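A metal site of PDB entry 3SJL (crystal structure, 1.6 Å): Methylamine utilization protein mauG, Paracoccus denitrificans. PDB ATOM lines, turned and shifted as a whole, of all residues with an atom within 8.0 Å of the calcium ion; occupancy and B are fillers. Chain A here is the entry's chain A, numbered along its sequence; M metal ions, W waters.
Water W3 bridges O of Gly 276 (3.1 Å) and ND2 of Asn 66 (3.3 Å).
Of the 21 residues printed, 3 come within 4 Å of the calcium ion.
Water W2 is bound to the calcium ion, at 2.2 Å.
The backbone carbonyl oxygen (O) of Pro 277 is bound to the calcium ion, at 2.3 Å.
The calcium ion is bound by O of Thr 275 (2.4 Å).
Water W4 binds the calcium ion (2.4 Å).
Water W1 binds the calcium ion, 2.4 Å away.
The calcium ion is bound by OD1 of Asn 66, 2.5 Å away.
Water W3 binds the calcium ion, 2.5 Å away.
The calcium ion has seven donor atoms within binding distance.
The backbone carbonyl oxygen (O) of Val 272 lies within hydrogen-bond range of the side-chain hydroxyl (OG1) of Thr 275.
The backbone NH of Asn 66 is in hydrogen-bond range of the backbone carbonyl oxygen of His 280 (2.8 Å).
NE1 of Trp 93 sits at hydrogen-bond distance from O of Asn 66, at 3.0 Å.
The side-chain hydroxyl (OG1) of Thr 275 sits close to the backbone carbonyl oxygen (O) of Asn 271.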
ATOM      1  N   ARG A  39     -15.679 -16.748  36.749  1.00  0.00           N
ATOM      2  CA  ARG A  39     -16.882 -15.962  36.426  1.00  0.00           C
ATOM      3  C   ARG A  39     -18.083 -16.878  36.323  1.00  0.00           C
ATOM      4  O   ARG A  39     -18.869 -16.809  35.353  1.00  0.00           O
ATOM      5  CB  ARG A  39     -16.755 -15.265  35.095  1.00  0.00           C
ATOM      6  CG  ARG A  39     -17.839 -14.181  34.904  1.00  0.00           C
ATOM      7  CD  ARG A  39     -17.500 -13.402  33.811  1.00  0.00           C
ATOM      8  NE  ARG A  39     -18.411 -12.307  33.722  1.00  0.00           N
ATOM      9  CZ  ARG A  39     -19.556 -12.281  33.050  1.00  0.00           C
ATOM     10  NH1 ARG A  39     -20.136 -11.142  33.097  1.00  0.00           N
ATOM     11  NH2 ARG A  39     -20.030 -13.322  32.235  1.00  0.00           N
ATOM     12  N   THR A  42     -18.755 -18.842  32.984  1.00  0.00           N
ATOM     13  CA  THR A  42     -19.192 -18.124  31.792  1.00  0.00           C
ATOM     14  C   THR A  42     -18.004 -17.328  31.313  1.00  0.00           C
ATOM     15  O   THR A  42     -16.914 -17.385  31.909  1.00  0.00           O
ATOM     16  CB  THR A  42     -20.351 -17.120  32.050  1.00  0.00           C
ATOM     17  OG1 THR A  42     -19.961 -16.159  33.023  1.00  0.00           O
ATOM     18  CG2 THR A  42     -21.592 -17.968  32.562  1.00  0.00           C
ATOM     19  N   ASP A  43     -18.233 -16.572  30.254  1.00  0.00           N
ATOM     20  CA  ASP A  43     -17.094 -15.951  29.569  1.00  0.00           C
ATOM     21  C   ASP A  43     -16.770 -14.550  30.112  1.00  0.00           C
ATOM     22  O   ASP A  43     -17.610 -13.670  29.910  1.00  0.00           O
ATOM     23  CB  ASP A  43     -17.395 -15.960  28.043  1.00  0.00           C
ATOM     24  CG  ASP A  43     -16.114 -15.568  27.207  1.00  0.00           C
ATOM     25  OD1 ASP A  43     -16.161 -15.920  25.969  1.00  0.00           O
ATOM     26  OD2 ASP A  43     -15.095 -14.990  27.777  1.00  0.00           O
ATOM     27  N   ASN A  66     -25.097 -16.631  23.397  1.00  0.00           N
ATOM     28  CA  ASN A  66     -24.327 -16.255  24.565  1.00  0.00           C
ATOM     29  C   ASN A  66     -23.909 -17.579  25.326  1.00  0.00           C
ATOM     30  O   ASN A  66     -24.637 -18.622  25.265  1.00  0.00           O
ATOM     31  CB  ASN A  66     -25.286 -15.447  25.455  1.00  0.00           C
ATOM     32  CG  ASN A  66     -24.548 -14.918  26.700  1.00  0.00           C
ATOM     33  OD1 ASN A  66     -24.854 -15.383  27.858  1.00  0.00           O
ATOM     34  ND2 ASN A  66     -23.549 -14.091  26.513  1.00  0.00           N
ATOM     35  N   THR A  67     -22.709 -17.552  25.923  1.00  0.00           N
ATOM     36  CA  THR A  67     -22.194 -18.718  26.621  1.00  0.00           C
ATOM     37  C   THR A  67     -22.859 -18.896  28.028  1.00  0.00           C
ATOM     38  O   THR A  67     -22.794 -17.989  28.894  1.00  0.00           O
ATOM     39  CB  THR A  67     -20.700 -18.626  26.816  1.00  0.00           C
ATOM     40  OG1 THR A  67     -20.129 -18.581  25.532  1.00  0.00           O
ATOM     41  CG2 THR A  67     -20.229 -19.799  27.570  1.00  0.00           C
ATOM     42  N   PRO A  68     -23.599 -19.952  28.210  1.00  0.00           N
ATOM     43  CA  PRO A  68     -24.283 -20.053  29.469  1.00  0.00           C
ATOM     44  C   PRO A  68     -23.407 -20.645  30.580  1.00  0.00           C
ATOM     45  O   PRO A  68     -22.422 -21.353  30.331  1.00  0.00           O
ATOM     46  CB  PRO A  68     -25.431 -21.103  29.128  1.00  0.00           C
ATOM     47  CG  PRO A  68     -24.763 -22.055  28.090  1.00  0.00           C
ATOM     48  CD  PRO A  68     -23.922 -21.078  27.252  1.00  0.00           C
ATOM     49  N   THR A  69     -23.829 -20.471  31.842  1.00  0.00           N
ATOM     50  CA  THR A  69     -23.103 -21.049  32.931  1.00  0.00           C
ATOM     51  C   THR A  69     -23.173 -22.536  33.002  1.00  0.00           C
ATOM     52  O   THR A  69     -24.251 -23.143  32.731  1.00  0.00           O
ATOM     53  CB  THR A  69     -23.647 -20.416  34.302  1.00  0.00           C
ATOM     54  OG1 THR A  69     -22.916 -20.914  35.444  1.00  0.00           O
ATOM     55  CG2 THR A  69     -25.162 -20.820  34.521  1.00  0.00           C
ATOM     56  N   TRP A  93     -29.000 -23.978  24.614  1.00  0.00           N
ATOM     57  CA  TRP A  93     -30.178 -23.105  24.639  1.00  0.00           C
ATOM     58  C   TRP A  93     -31.357 -23.743  23.904  1.00  0.00           C
ATOM     59  O   TRP A  93     -32.499 -23.373  24.226  1.00  0.00           O
ATOM     60  CB  TRP A  93     -29.874 -21.722  24.054  1.00  0.00           C
ATOM     61  CG  TRP A  93     -29.080 -20.842  24.951  1.00  0.00           C
ATOM     62  CD1 TRP A  93     -27.689 -20.566  24.863  1.00  0.00           C
ATOM     63  CD2 TRP A  93     -29.606 -19.987  26.008  1.00  0.00           C
ATOM     64  NE1 TRP A  93     -27.360 -19.643  25.863  1.00  0.00           N
ATOM     65  CE2 TRP A  93     -28.488 -19.244  26.525  1.00  0.00           C
ATOM     66  CE3 TRP A  93     -30.903 -19.778  26.564  1.00  0.00           C
ATOM     67  CZ2 TRP A  93     -28.625 -18.290  27.593  1.00  0.00           C
ATOM     68  CZ3 TRP A  93     -30.992 -18.783  27.678  1.00  0.00           C
ATOM     69  CH2 TRP A  93     -29.904 -18.102  28.093  1.00  0.00           C
ATOM     70  N   ASN A 271     -26.536 -17.455  40.236  1.00  0.00           N
ATOM     71  CA  ASN A 271     -25.364 -16.591  39.752  1.00  0.00           C
ATOM     72  C   ASN A 271     -25.746 -15.592  38.650  1.00  0.00           C
ATOM     73  O   ASN A 271     -24.879 -15.039  38.025  1.00  0.00           O
ATOM     74  CB  ASN A 271     -24.194 -17.436  39.257  1.00  0.00           C
ATOM     75  CG  ASN A 271     -23.517 -18.186  40.432  1.00  0.00           C
ATOM     76  OD1 ASN A 271     -23.239 -17.553  41.444  1.00  0.00           O
ATOM     77  ND2 ASN A 271     -23.341 -19.513  40.287  1.00  0.00           N
ATOM     78  N   VAL A 272     -27.055 -15.398  38.401  1.00  0.00           N
ATOM     79  CA  VAL A 272     -27.414 -14.483  37.320  1.00  0.00           C
ATOM     80  C   VAL A 272     -26.748 -13.090  37.457  1.00  0.00           C
ATOM     81  O   VAL A 272     -26.429 -12.487  36.441  1.00  0.00           O
ATOM     82  CB  VAL A 272     -29.008 -14.409  37.169  1.00  0.00           C
ATOM     83  CG1 VAL A 272     -29.632 -13.608  38.338  1.00  0.00           C
ATOM     84  CG2 VAL A 272     -29.338 -13.744  35.828  1.00  0.00           C
ATOM     85  N   VAL A 274     -23.923 -12.227  38.104  1.00  0.00           N
ATOM     86  CA  VAL A 274     -22.502 -12.110  37.697  1.00  0.00           C
ATOM     87  C   VAL A 274     -22.237 -12.712  36.298  1.00  0.00           C
ATOM     88  O   VAL A 274     -21.081 -12.746  35.827  1.00  0.00           O
ATOM     89  CB  VAL A 274     -21.557 -12.764  38.788  1.00  0.00           C
ATOM     90  CG1 VAL A 274     -21.745 -12.044  40.163  1.00  0.00           C
ATOM     91  CG2 VAL A 274     -21.770 -14.239  38.921  1.00  0.00           C
ATOM     92  N   THR A 275     -23.295 -13.108  35.597  1.00  0.00           N
ATOM     93  CA  THR A 275     -23.096 -13.764  34.291  1.00  0.00           C
ATOM     94  C   THR A 275     -23.655 -12.996  33.080  1.00  0.00           C
ATOM     95  O   THR A 275     -24.011 -13.612  32.065  1.00  0.00           O
ATOM     96  CB  THR A 275     -23.701 -15.135  34.290  1.00  0.00           C
ATOM     97  OG1 THR A 275     -25.114 -15.026  34.643  1.00  0.00           O
ATOM     98  CG2 THR A 275     -22.993 -16.034  35.408  1.00  0.00           C
ATOM     99  N   GLY A 276     -23.726 -11.664  33.174  1.00  0.00           N
ATOM    100  CA  GLY A 276     -24.182 -10.886  32.006  1.00  0.00           C
ATOM    101  C   GLY A 276     -23.133 -11.070  30.862  1.00  0.00           C
ATOM    102  O   GLY A 276     -21.954 -11.402  31.094  1.00  0.00           O
ATOM    103  N   PRO A 277     -23.527 -10.787  29.644  1.00  0.00           N
ATOM    104  CA  PRO A 277     -24.891 -10.282  29.305  1.00  0.00           C
ATOM    105  C   PRO A 277     -25.901 -11.398  29.250  1.00  0.00           C
ATOM    106  O   PRO A 277     -25.620 -12.602  29.459  1.00  0.00           O
ATOM    107  CB  PRO A 277     -24.717  -9.712  27.904  1.00  0.00           C
ATOM    108  CG  PRO A 277     -23.524 -10.522  27.305  1.00  0.00           C
ATOM    109  CD  PRO A 277     -22.606 -10.807  28.459  1.00  0.00           C
ATOM    110  N   TYR A 278     -27.129 -10.966  28.999  1.00  0.00           N
ATOM    111  CA  TYR A 278     -28.236 -11.849  29.276  1.00  0.00           C
ATOM    112  C   TYR A 278     -29.017 -12.290  28.049  1.00  0.00           C
ATOM    113  O   TYR A 278     -29.004 -11.593  26.988  1.00  0.00           O
ATOM    114  CB  TYR A 278     -29.166 -11.169  30.301  1.00  0.00           C
ATOM    115  CG  TYR A 278     -28.433 -10.860  31.541  1.00  0.00           C
ATOM    116  CD1 TYR A 278     -27.917  -9.576  31.802  1.00  0.00           C
ATOM    117  CD2 TYR A 278     -28.182 -11.879  32.471  1.00  0.00           C
ATOM    118  CE1 TYR A 278     -27.203  -9.318  32.974  1.00  0.00           C
ATOM    119  CE2 TYR A 278     -27.490 -11.638  33.606  1.00  0.00           C
ATOM    120  CZ  TYR A 278     -26.952 -10.346  33.860  1.00  0.00           C
ATOM    121  OH  TYR A 278     -26.264 -10.160  35.042  1.00  0.00           O
ATOM    122  N   MET A 279     -29.774 -13.367  28.277  1.00  0.00           N
ATOM    123  CA  MET A 279     -30.662 -14.083  27.238  1.00  0.00           C
ATOM    124  C   MET A 279     -29.806 -14.869  26.230  1.00  0.00           C
ATOM    125  O   MET A 279     -28.561 -14.774  26.289  1.00  0.00           O
ATOM    126  CB  MET A 279     -31.573 -13.058  26.497  1.00  0.00           C
ATOM    127  CG  MET A 279     -32.401 -12.098  27.471  1.00  0.00           C
ATOM    128  SD  MET A 279     -33.513 -13.227  28.399  1.00  0.00           S
ATOM    129  CE  MET A 279     -34.242 -11.966  29.512  1.00  0.00           C
ATOM    130  N   HIS A 280     -30.466 -15.637  25.365  1.00  0.00           N
ATOM    131  CA  HIS A 280     -29.770 -16.568  24.532  1.00  0.00           C
ATOM    132  C   HIS A 280     -28.749 -15.923  23.583  1.00  0.00           C
ATOM    133  O   HIS A 280     -27.851 -16.598  23.127  1.00  0.00           O
ATOM    134  CB  HIS A 280     -30.782 -17.478  23.784  1.00  0.00           C
ATOM    135  CG  HIS A 280     -31.600 -16.748  22.746  1.00  0.00           C
ATOM    136  ND1 HIS A 280     -32.923 -16.340  22.947  1.00  0.00           N
ATOM    137  CD2 HIS A 280     -31.231 -16.287  21.521  1.00  0.00           C
ATOM    138  CE1 HIS A 280     -33.306 -15.629  21.893  1.00  0.00           C
ATOM    139  NE2 HIS A 280     -32.318 -15.618  21.002  1.00  0.00           N
ATOM    140  N   ASN A 281     -28.938 -14.639  23.289  1.00  0.00           N
ATOM    141  CA  ASN A 281     -28.115 -13.967  22.307  1.00  0.00           C
ATOM    142  C   ASN A 281     -27.356 -12.818  22.949  1.00  0.00           C
ATOM    143  O   ASN A 281     -26.836 -11.987  22.219  1.00  0.00           O
ATOM    144  CB  ASN A 281     -29.010 -13.477  21.158  1.00  0.00           C
ATOM    145  CG  ASN A 281     -30.160 -12.534  21.629  1.00  0.00           C
ATOM    146  OD1 ASN A 281     -30.255 -12.188  22.801  1.00  0.00           O
ATOM    147  ND2 ASN A 281     -31.106 -12.291  20.722  1.00  0.00           N
ATOM    148  N   GLY A 282     -27.448 -12.713  24.297  1.00  0.00           N
ATOM    149  CA  GLY A 282     -26.622 -11.676  24.989  1.00  0.00           C
ATOM    150  C   GLY A 282     -27.073 -10.271  24.713  1.00  0.00           C
ATOM    151  O   GLY A 282     -26.276  -9.317  24.892  1.00  0.00           O
ATOM    152  N   PHE A 284     -29.039  -8.060  26.218  1.00  0.00           N
ATOM    153  CA  PHE A 284     -29.058  -7.033  27.285  1.00  0.00           C
ATOM    154  C   PHE A 284     -27.857  -7.140  28.169  1.00  0.00           C
ATOM    155  O   PHE A 284     -27.522  -8.226  28.673  1.00  0.00           O
ATOM    156  CB  PHE A 284     -30.247  -7.270  28.181  1.00  0.00           C
ATOM    157  CG  PHE A 284     -31.569  -7.369  27.439  1.00  0.00           C
ATOM    158  CD1 PHE A 284     -31.844  -6.490  26.387  1.00  0.00           C
ATOM    159  CD2 PHE A 284     -32.484  -8.351  27.781  1.00  0.00           C
ATOM    160  CE1 PHE A 284     -32.969  -6.522  25.682  1.00  0.00           C
ATOM    161  CE2 PHE A 284     -33.696  -8.409  27.081  1.00  0.00           C
ATOM    162  CZ  PHE A 284     -33.981  -7.472  26.054  1.00  0.00           C
ATOM    163  N   THR A 285     -27.174  -6.037  28.387  1.00  0.00           N
ATOM    164  CA  THR A 285     -25.959  -6.151  29.136  1.00  0.00           C
ATOM    165  C   THR A 285     -26.181  -6.151  30.651  1.00  0.00           C
ATOM    166  O   THR A 285     -25.426  -6.803  31.382  1.00  0.00           O
ATOM    167  CB  THR A 285     -25.021  -4.968  28.776  1.00  0.00           C
ATOM    168  OG1 THR A 285     -25.604  -3.762  29.266  1.00  0.00           O
ATOM    169  CG2 THR A 285     -24.770  -4.830  27.279  1.00  0.00           C
HETATM  170 CA    CA M   1     -25.049 -14.657  30.231  1.00  0.00          CA
HETATM  171  O   HOH W   1     -27.166 -15.365  29.286  1.00  0.00           O
HETATM  172  O   HOH W   2     -24.246 -16.663  30.818  1.00  0.00           O
HETATM  173  O   HOH W   3     -22.670 -14.041  29.702  1.00  0.00           O
HETATM  174  O   HOH W   4     -26.443 -15.008  32.094  1.00  0.00           O
